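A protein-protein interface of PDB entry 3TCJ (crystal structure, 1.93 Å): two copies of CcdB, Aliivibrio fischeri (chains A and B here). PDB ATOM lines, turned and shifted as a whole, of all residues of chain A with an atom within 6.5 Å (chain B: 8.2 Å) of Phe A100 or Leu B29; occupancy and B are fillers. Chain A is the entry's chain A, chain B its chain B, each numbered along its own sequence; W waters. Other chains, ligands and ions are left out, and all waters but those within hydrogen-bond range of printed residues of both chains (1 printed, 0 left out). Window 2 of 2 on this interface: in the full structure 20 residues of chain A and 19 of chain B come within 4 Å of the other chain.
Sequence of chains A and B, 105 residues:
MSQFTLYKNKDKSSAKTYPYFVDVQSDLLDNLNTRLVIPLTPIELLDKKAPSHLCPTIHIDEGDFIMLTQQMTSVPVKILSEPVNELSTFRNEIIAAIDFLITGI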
ATOM      1  N   PRO A  51     -13.502   2.605  29.179  1.00  0.00           N
ATOM      2  CA  PRO A  51     -13.357   2.664  27.720  1.00  0.00           C
ATOM      3  C   PRO A  51     -14.702   2.961  27.066  1.00  0.00           C
ATOM      4  O   PRO A  51     -15.627   2.160  27.189  1.00  0.00           O
ATOM      5  CB  PRO A  51     -12.887   1.246  27.362  1.00  0.00           C
ATOM      6  CG  PRO A  51     -13.260   0.407  28.569  1.00  0.00           C
ATOM      7  CD  PRO A  51     -13.011   1.326  29.714  1.00  0.00           C
ATOM      8  N   HIS A  53     -15.831   3.008  24.018  1.00  0.00           N
ATOM      9  CA  HIS A  53     -16.304   2.131  22.951  1.00  0.00           C
ATOM     10  C   HIS A  53     -17.081   0.954  23.535  1.00  0.00           C
ATOM     11  O   HIS A  53     -18.028   0.463  22.926  1.00  0.00           O
ATOM     12  CB  HIS A  53     -15.131   1.641  22.094  1.00  0.00           C
ATOM     13  CG  HIS A  53     -15.544   1.027  20.791  1.00  0.00           C
ATOM     14  ND1 HIS A  53     -16.310   1.696  19.862  1.00  0.00           N
ATOM     15  CD2 HIS A  53     -15.278  -0.188  20.255  1.00  0.00           C
ATOM     16  CE1 HIS A  53     -16.510   0.915  18.815  1.00  0.00           C
ATOM     17  NE2 HIS A  53     -15.893  -0.232  19.028  1.00  0.00           N
ATOM     18  N   LEU A  54     -16.682   0.516  24.725  1.00  0.00           N
ATOM     19  CA  LEU A  54     -17.332  -0.605  25.399  1.00  0.00           C
ATOM     20  C   LEU A  54     -18.388  -0.128  26.391  1.00  0.00           C
ATOM     21  O   LEU A  54     -19.435  -0.753  26.547  1.00  0.00           O
ATOM     22  CB  LEU A  54     -16.298  -1.463  26.132  1.00  0.00           C
ATOM     23  CG  LEU A  54     -16.853  -2.610  26.978  1.00  0.00           C
ATOM     24  CD1 LEU A  54     -17.471  -3.684  26.090  1.00  0.00           C
ATOM     25  CD2 LEU A  54     -15.771  -3.205  27.866  1.00  0.00           C
ATOM     26  N   CYS A  55     -18.100   0.980  27.065  1.00  0.00           N
ATOM     27  CA  CYS A  55     -18.982   1.492  28.105  1.00  0.00           C
ATOM     28  C   CYS A  55     -19.375   2.934  27.814  1.00  0.00           C
ATOM     29  O   CYS A  55     -18.836   3.861  28.414  1.00  0.00           O
ATOM     30  CB  CYS A  55     -18.297   1.405  29.469  1.00  0.00           C
ATOM     31  SG  CYS A  55     -17.606  -0.223  29.857  1.00  0.00           S
ATOM     32  N   ILE A  95     -25.885  -1.368  20.898  1.00  0.00           N
ATOM     33  CA  ILE A  95     -25.619  -2.565  20.111  1.00  0.00           C
ATOM     34  C   ILE A  95     -24.137  -2.673  19.767  1.00  0.00           C
ATOM     35  O   ILE A  95     -23.545  -3.750  19.857  1.00  0.00           O
ATOM     36  CB  ILE A  95     -26.444  -2.579  18.813  1.00  0.00           C
ATOM     37  CG1 ILE A  95     -27.937  -2.517  19.132  1.00  0.00           C
ATOM     38  CG2 ILE A  95     -26.127  -3.819  17.992  1.00  0.00           C
ATOM     39  CD1 ILE A  95     -28.407  -3.624  20.039  1.00  0.00           C
ATOM     40  N   ALA A  96     -23.543  -1.550  19.375  1.00  0.00           N
ATOM     41  CA  ALA A  96     -22.129  -1.515  19.016  1.00  0.00           C
ATOM     42  C   ALA A  96     -21.251  -1.853  20.216  1.00  0.00           C
ATOM     43  O   ALA A  96     -20.177  -2.435  20.065  1.00  0.00           O
ATOM     44  CB  ALA A  96     -21.759  -0.156  18.451  1.00  0.00           C
ATOM     45  N   ALA A  97     -21.713  -1.483  21.407  1.00  0.00           N
ATOM     46  CA  ALA A  97     -20.986  -1.786  22.634  1.00  0.00           C
ATOM     47  C   ALA A  97     -20.971  -3.289  22.888  1.00  0.00           C
ATOM     48  O   ALA A  97     -19.931  -3.870  23.202  1.00  0.00           O
ATOM     49  CB  ALA A  97     -21.607  -1.051  23.815  1.00  0.00           C
ATOM     50  N   ILE A  98     -22.135  -3.915  22.756  1.00  0.00           N
ATOM     51  CA  ILE A  98     -22.248  -5.359  22.913  1.00  0.00           C
ATOM     52  C   ILE A  98     -21.419  -6.082  21.853  1.00  0.00           C
ATOM     53  O   ILE A  98     -20.698  -7.035  22.156  1.00  0.00           O
ATOM     54  CB  ILE A  98     -23.713  -5.812  22.804  1.00  0.00           C
ATOM     55  CG1 ILE A  98     -24.551  -5.175  23.922  1.00  0.00           C
ATOM     56  CG2 ILE A  98     -23.799  -7.322  22.864  1.00  0.00           C
ATOM     57  CD1 ILE A  98     -26.048  -5.358  23.753  1.00  0.00           C
ATOM     58  N   ASP A  99     -21.524  -5.619  20.611  1.00  0.00           N
ATOM     59  CA  ASP A  99     -20.768  -6.211  19.513  1.00  0.00           C
ATOM     60  C   ASP A  99     -19.269  -6.109  19.757  1.00  0.00           C
ATOM     61  O   ASP A  99     -18.520  -7.034  19.449  1.00  0.00           O
ATOM     62  CB  ASP A  99     -21.133  -5.544  18.188  1.00  0.00           C
ATOM     63  CG  ASP A  99     -22.517  -5.935  17.698  1.00  0.00           C
ATOM     64  OD1 ASP A  99     -23.114  -6.863  18.281  1.00  0.00           O
ATOM     65  OD2 ASP A  99     -23.001  -5.314  16.732  1.00  0.00           O
ATOM     66  N   PHE A 100     -18.837  -4.981  20.309  1.00  0.00           N
ATOM     67  CA  PHE A 100     -17.432  -4.784  20.645  1.00  0.00           C
ATOM     68  C   PHE A 100     -16.987  -5.804  21.686  1.00  0.00           C
ATOM     69  O   PHE A 100     -15.916  -6.401  21.572  1.00  0.00           O
ATOM     70  CB  PHE A 100     -17.207  -3.361  21.161  1.00  0.00           C
ATOM     71  CG  PHE A 100     -15.774  -3.053  21.494  1.00  0.00           C
ATOM     72  CD1 PHE A 100     -14.763  -3.313  20.584  1.00  0.00           C
ATOM     73  CD2 PHE A 100     -15.442  -2.480  22.710  1.00  0.00           C
ATOM     74  CE1 PHE A 100     -13.444  -3.021  20.889  1.00  0.00           C
ATOM     75  CE2 PHE A 100     -14.125  -2.183  23.021  1.00  0.00           C
ATOM     76  CZ  PHE A 100     -13.127  -2.454  22.109  1.00  0.00           C
ATOM     77  N   LEU A 101     -17.827  -6.006  22.696  1.00  0.00           N
ATOM     78  CA  LEU A 101     -17.541  -6.938  23.780  1.00  0.00           C
ATOM     79  C   LEU A 101     -17.256  -8.354  23.279  1.00  0.00           C
ATOM     80  O   LEU A 101     -16.446  -9.073  23.863  1.00  0.00           O
ATOM     81  CB  LEU A 101     -18.711  -6.965  24.768  1.00  0.00           C
ATOM     82  CG  LEU A 101     -18.566  -7.875  25.990  1.00  0.00           C
ATOM     83  CD1 LEU A 101     -17.339  -7.494  26.804  1.00  0.00           C
ATOM     84  CD2 LEU A 101     -19.824  -7.826  26.847  1.00  0.00           C
ATOM     85  N   ILE A 102     -17.921  -8.750  22.198  1.00  0.00           N
ATOM     86  CA  ILE A 102     -17.808 -10.120  21.703  1.00  0.00           C
ATOM     87  C   ILE A 102     -17.027 -10.255  20.395  1.00  0.00           C
ATOM     88  O   ILE A 102     -16.901 -11.357  19.863  1.00  0.00           O
ATOM     89  CB  ILE A 102     -19.199 -10.762  21.507  1.00  0.00           C
ATOM     90  CG1 ILE A 102     -19.971 -10.040  20.397  1.00  0.00           C
ATOM     91  CG2 ILE A 102     -19.983 -10.747  22.807  1.00  0.00           C
ATOM     92  CD1 ILE A 102     -21.390 -10.540  20.213  1.00  0.00           C
ATOM     93  N   THR A 103     -16.499  -9.149  19.877  1.00  0.00           N
ATOM     94  CA  THR A 103     -15.784  -9.177  18.603  1.00  0.00           C
ATOM     95  C   THR A 103     -14.486  -8.377  18.639  1.00  0.00           C
ATOM     96  O   THR A 103     -13.545  -8.670  17.900  1.00  0.00           O
ATOM     97  CB  THR A 103     -16.659  -8.646  17.453  1.00  0.00           C
ATOM     98  OG1 THR A 103     -16.579  -7.216  17.409  1.00  0.00           O
ATOM     99  N   GLY A 104     -14.438  -7.362  19.495  1.00  0.00           N
ATOM    100  CA  GLY A 104     -13.275  -6.499  19.574  1.00  0.00           C
ATOM    101  C   GLY A 104     -13.271  -5.491  18.442  1.00  0.00           C
ATOM    102  O   GLY A 104     -12.279  -4.800  18.215  1.00  0.00           O
ATOM    103  N   ILE A 105     -14.387  -5.419  17.724  1.00  0.00           N
ATOM    104  CA  ILE A 105     -14.557  -4.448  16.652  1.00  0.00           C
ATOM    105  C   ILE A 105     -15.430  -3.292  17.126  1.00  0.00           C
ATOM    106  O   ILE A 105     -15.120  -2.122  16.905  1.00  0.00           O
ATOM    107  CB  ILE A 105     -15.214  -5.084  15.413  1.00  0.00           C
ATOM    108  CG1 ILE A 105     -14.316  -6.174  14.828  1.00  0.00           C
ATOM    109  CG2 ILE A 105     -15.519  -4.021  14.367  1.00  0.00           C
ATOM    110  CD1 ILE A 105     -14.909  -6.859  13.620  1.00  0.00           C
ATOM    111  OXT ILE A 105     -16.469  -3.507  17.749  1.00  0.00           O
ATOM    112  N   GLN B   3     -11.282 -16.656  24.032  1.00  0.00           N
ATOM    113  CA  GLN B   3     -12.670 -16.621  23.602  1.00  0.00           C
ATOM    114  C   GLN B   3     -12.984 -17.978  22.984  1.00  0.00           C
ATOM    115  O   GLN B   3     -12.175 -18.518  22.227  1.00  0.00           O
ATOM    116  CB  GLN B   3     -12.886 -15.506  22.578  1.00  0.00           C
ATOM    117  CG  GLN B   3     -14.330 -15.329  22.133  1.00  0.00           C
ATOM    118  CD  GLN B   3     -14.483 -14.262  21.067  1.00  0.00           C
ATOM    119  OE1 GLN B   3     -13.608 -14.087  20.218  1.00  0.00           O
ATOM    120  NE2 GLN B   3     -15.600 -13.544  21.104  1.00  0.00           N
ATOM    121  N   VAL B  24     -17.354 -16.175  25.729  1.00  0.00           N
ATOM    122  CA  VAL B  24     -17.689 -15.578  24.440  1.00  0.00           C
ATOM    123  C   VAL B  24     -17.158 -14.154  24.315  1.00  0.00           C
ATOM    124  O   VAL B  24     -17.472 -13.447  23.359  1.00  0.00           O
ATOM    125  CB  VAL B  24     -19.211 -15.578  24.192  1.00  0.00           C
ATOM    126  CG1 VAL B  24     -19.727 -17.007  24.045  1.00  0.00           C
ATOM    127  CG2 VAL B  24     -19.935 -14.844  25.314  1.00  0.00           C
ATOM    128  N   GLN B  25     -16.346 -13.749  25.284  1.00  0.00           N
ATOM    129  CA  GLN B  25     -15.807 -12.395  25.323  1.00  0.00           C
ATOM    130  C   GLN B  25     -14.545 -12.262  24.472  1.00  0.00           C
ATOM    131  O   GLN B  25     -13.720 -13.173  24.418  1.00  0.00           O
ATOM    132  CB  GLN B  25     -15.521 -11.989  26.769  1.00  0.00           C
ATOM    133  CG  GLN B  25     -14.970 -10.586  26.938  1.00  0.00           C
ATOM    134  CD  GLN B  25     -14.952 -10.147  28.389  1.00  0.00           C
ATOM    135  OE1 GLN B  25     -13.904  -9.793  28.931  1.00  0.00           O
ATOM    136  NE2 GLN B  25     -16.114 -10.183  29.030  1.00  0.00           N
ATOM    137  N   SER B  26     -14.404 -11.120  23.807  1.00  0.00           N
ATOM    138  CA  SER B  26     -13.259 -10.869  22.938  1.00  0.00           C
ATOM    139  C   SER B  26     -11.943 -10.869  23.711  1.00  0.00           C
ATOM    140  O   SER B  26     -11.860 -10.338  24.817  1.00  0.00           O
ATOM    141  CB  SER B  26     -13.430  -9.542  22.196  1.00  0.00           C
ATOM    142  OG  SER B  26     -12.221  -9.154  21.566  1.00  0.00           O
ATOM    143  N   ASP B  27     -10.917 -11.467  23.115  1.00  0.00           N
ATOM    144  CA  ASP B  27      -9.597 -11.534  23.734  1.00  0.00           C
ATOM    145  C   ASP B  27      -8.974 -10.150  23.888  1.00  0.00           C
ATOM    146  O   ASP B  27      -8.104  -9.942  24.734  1.00  0.00           O
ATOM    147  CB  ASP B  27      -8.674 -12.445  22.922  1.00  0.00           C
ATOM    148  CG  ASP B  27      -9.082 -13.902  23.003  1.00  0.00           C
ATOM    149  OD1 ASP B  27      -9.698 -14.286  24.019  1.00  0.00           O
ATOM    150  OD2 ASP B  27      -8.794 -14.659  22.055  1.00  0.00           O
ATOM    151  N   LEU B  28      -9.422  -9.206  23.065  1.00  0.00           N
ATOM    152  CA  LEU B  28      -8.944  -7.830  23.147  1.00  0.00           C
ATOM    153  C   LEU B  28      -9.264  -7.199  24.497  1.00  0.00           C
ATOM    154  O   LEU B  28      -8.587  -6.269  24.931  1.00  0.00           O
ATOM    155  CB  LEU B  28      -9.544  -6.983  22.023  1.00  0.00           C
ATOM    156  CG  LEU B  28      -8.733  -6.876  20.731  1.00  0.00           C
ATOM    157  CD2 LEU B  28      -7.439  -6.114  20.984  1.00  0.00           C
ATOM    158  N   LEU B  29     -10.299  -7.709  25.157  1.00  0.00           N
ATOM    159  CA  LEU B  29     -10.756  -7.135  26.418  1.00  0.00           C
ATOM    160  C   LEU B  29     -10.428  -8.026  27.612  1.00  0.00           C
ATOM    161  O   LEU B  29     -11.117  -7.991  28.630  1.00  0.00           O
ATOM    162  CB  LEU B  29     -12.262  -6.872  26.364  1.00  0.00           C
ATOM    163  CG  LEU B  29     -12.747  -6.021  25.189  1.00  0.00           C
ATOM    164  CD1 LEU B  29     -14.264  -6.022  25.107  1.00  0.00           C
ATOM    165  CD2 LEU B  29     -12.210  -4.599  25.295  1.00  0.00           C
ATOM    166  N   ASP B  30      -9.366  -8.814  27.489  1.00  0.00           N
ATOM    167  CA  ASP B  30      -9.004  -9.765  28.535  1.00  0.00           C
ATOM    168  C   ASP B  30      -8.429  -9.088  29.778  1.00  0.00           C
ATOM    169  O   ASP B  30      -8.160  -9.749  30.781  1.00  0.00           O
ATOM    170  CB  ASP B  30      -8.032 -10.818  27.998  1.00  0.00           C
ATOM    171  CG  ASP B  30      -6.670 -10.244  27.662  1.00  0.00           C
ATOM    172  OD1 ASP B  30      -6.527  -9.003  27.617  1.00  0.00           O
ATOM    173  OD2 ASP B  30      -5.737 -11.043  27.441  1.00  0.00           O
ATOM    174  N   ASN B  31      -8.240  -7.775  29.708  1.00  0.00           N
ATOM    175  CA  ASN B  31      -7.775  -7.016  30.863  1.00  0.00           C
ATOM    176  C   ASN B  31      -8.884  -6.843  31.895  1.00  0.00           C
ATOM    177  O   ASN B  31      -8.621  -6.547  33.060  1.00  0.00           O
ATOM    178  CB  ASN B  31      -7.229  -5.652  30.434  1.00  0.00           C
ATOM    179  N   LEU B  32     -10.125  -7.030  31.456  1.00  0.00           N
ATOM    180  CA  LEU B  32     -11.274  -6.967  32.351  1.00  0.00           C
ATOM    181  C   LEU B  32     -11.194  -8.083  33.382  1.00  0.00           C
ATOM    182  O   LEU B  32     -10.641  -9.147  33.110  1.00  0.00           O
ATOM    183  CB  LEU B  32     -12.577  -7.089  31.561  1.00  0.00           C
ATOM    184  CG  LEU B  32     -12.873  -6.004  30.526  1.00  0.00           C
ATOM    185  CD1 LEU B  32     -14.126  -6.352  29.735  1.00  0.00           C
ATOM    186  CD2 LEU B  32     -13.018  -4.651  31.201  1.00  0.00           C
ATOM    187  N   ASN B  33     -11.747  -7.842  34.566  1.00  0.00           N
ATOM    188  CA  ASN B  33     -11.753  -8.854  35.616  1.00  0.00           C
ATOM    189  C   ASN B  33     -13.025  -9.698  35.604  1.00  0.00           C
ATOM    190  O   ASN B  33     -13.301 -10.438  36.546  1.00  0.00           O
ATOM    191  CB  ASN B  33     -11.528  -8.218  36.992  1.00  0.00           C
ATOM    192  CG  ASN B  33     -12.529  -7.121  37.301  1.00  0.00           C
ATOM    193  OD1 ASN B  33     -13.718  -7.247  37.009  1.00  0.00           O
ATOM    194  ND2 ASN B  33     -12.052  -6.038  37.906  1.00  0.00           N
ATOM    195  N   THR B  34     -13.796  -9.577  34.528  1.00  0.00           N
ATOM    196  CA  THR B  34     -14.992 -10.388  34.344  1.00  0.00           C
ATOM    197  C   THR B  34     -15.033 -10.947  32.927  1.00  0.00           C
ATOM    198  O   THR B  34     -14.341 -10.454  32.035  1.00  0.00           O
ATOM    199  CB  THR B  34     -16.281  -9.582  34.604  1.00  0.00           C
ATOM    200  OG1 THR B  34     -16.339  -8.466  33.708  1.00  0.00           O
ATOM    201  CG2 THR B  34     -16.321  -9.078  36.042  1.00  0.00           C
ATOM    202  N   ARG B  35     -15.849 -11.976  32.726  1.00  0.00           N
ATOM    203  CA  ARG B  35     -15.981 -12.606  31.419  1.00  0.00           C
ATOM    204  C   ARG B  35     -17.440 -12.889  31.101  1.00  0.00           C
ATOM    205  O   ARG B  35     -18.188 -13.368  31.954  1.00  0.00           O
ATOM    206  CB  ARG B  35     -15.191 -13.916  31.375  1.00  0.00           C
ATOM    207  CG  ARG B  35     -13.690 -13.754  31.522  1.00  0.00           C
ATOM    208  CD  ARG B  35     -13.054 -13.217  30.250  1.00  0.00           C
ATOM    209  NE  ARG B  35     -11.598 -13.167  30.359  1.00  0.00           N
ATOM    210  CZ  ARG B  35     -10.925 -12.155  30.897  1.00  0.00           C
ATOM    211  NH1 ARG B  35     -11.579 -11.106  31.373  1.00  0.00           N
ATOM    212  NH2 ARG B  35      -9.601 -12.190  30.957  1.00  0.00           N
ATOM    213  N   VAL B  77     -13.659 -13.424  36.552  1.00  0.00           N
ATOM    214  CA  VAL B  77     -12.665 -14.193  35.813  1.00  0.00           C
ATOM    215  C   VAL B  77     -12.128 -15.344  36.661  1.00  0.00           C
ATOM    216  O   VAL B  77     -11.513 -16.275  36.141  1.00  0.00           O
ATOM    217  CB  VAL B  77     -11.491 -13.306  35.356  1.00  0.00           C
ATOM    218  CG1 VAL B  77     -10.542 -13.037  36.518  1.00  0.00           C
ATOM    219  CG2 VAL B  77     -10.749 -13.959  34.201  1.00  0.00           C
HETATM  220  O   HOH W   1     -11.870 -10.314  19.214  1.00  0.00           O
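The backbone carbonyl oxygen (O) of Leu A101 sits at hydrogen-bond distance from the backbone NH (N) of Ser B26, at 2.9 Å. O of Ile A102 lies within hydrogen-bond range of NE2 of Gln B3.
O of Asp A99 lies within hydrogen-bond range of OG1 of Thr A103, 2.8 Å away. N of Ile A105 is in hydrogen-bond range of OG1 of Thr A103 (2.9 Å). The side-chain amide nitrogen (NE2) of Gln B3 lies within hydrogen-bond range of the backbone carbonyl oxygen (O) of Val B24 (2.9 Å). N of Gln B3 is in hydrogen-bond range of OD1 of Asp B27 (2.9 Å). O of Leu B29 lies close to OE1 of Gln B25 (3.3 Å). The side-chain amide oxygen of Gln B25 lies close to the backbone carbonyl oxygen of Thr B34 (3.2 Å).
Leu B29 touches Phe A100. Gln B25 touches Leu A101 (CA to O, 3.7 Å). Leu A101 touches Leu B29 (CA to CD1, 3.7 Å). Val B24 touches Ile A102 (O to CB, 3.7 Å). Thr A103 touches Ser B26 (C to OG, 3.8 Å). CA of Gly A104 touches OG of Ser B26, 3.5 Å away.
Phe A100 touches just one residue of chain B: Leu B29 (3.8 Å). Leu B29 touches just these residues of chain A: Phe A100 (3.8 Å) and Leu A101 (3.7 Å). Of chain B, only Ser B26 (3.5 Å) comes within 4 Å of Gly A104. Of the printed residues of chain A, Gln B3 touches Ile A102. Printed residues of chain A within 4 Å of Gln B25: Leu A101 (3.7 Å). Of the printed residues of chain B, Ile A102 touches Gln B3 and Val B24. Of the printed residues of chain A, Ser B26 touches Leu A101, Thr A103 and Gly A104. Pro A51 touches none of the printed residues of chain B. The nearest residue of chain B that does not touch Phe A100 is Ser B26 (4.1 Å). The nearest printed residue of chain A that does not touch Val B24 is Leu A101 (4.5 Å).
Printed residues of chain A that touch a printed residue of chain B: Phe A100, Leu A101, Ile A102, Thr A103 and Gly A104. Hydrophobic or aromatic side chains of chain A that line the printed part of chain B: Phe A100, Leu A101 and Ile A102. Along chain A the printed residues that touch a printed residue of chain B span positions 100 to 104. Of the 14 printed residues of chain B, 5 touch a printed residue of chain A. Hydrophobic or aromatic side chains of chain B within 4 Å of the printed part of chain A: Leu B29. Among the printed residues, 8 pairs touch across the chains. Among the printed residues, no Asp or Glu carboxylate lies within 4 Å of a Lys or Arg side-chain nitrogen of the other chain.
No position is printed for both chains. Of the 8 pairs that touch across the chains among the printed residues, none has its exchanged pair printed and touching as well.
Water W1 bridges the side-chain hydroxyl of Ser B26 and the backbone carbonyl oxygen of Thr A103.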
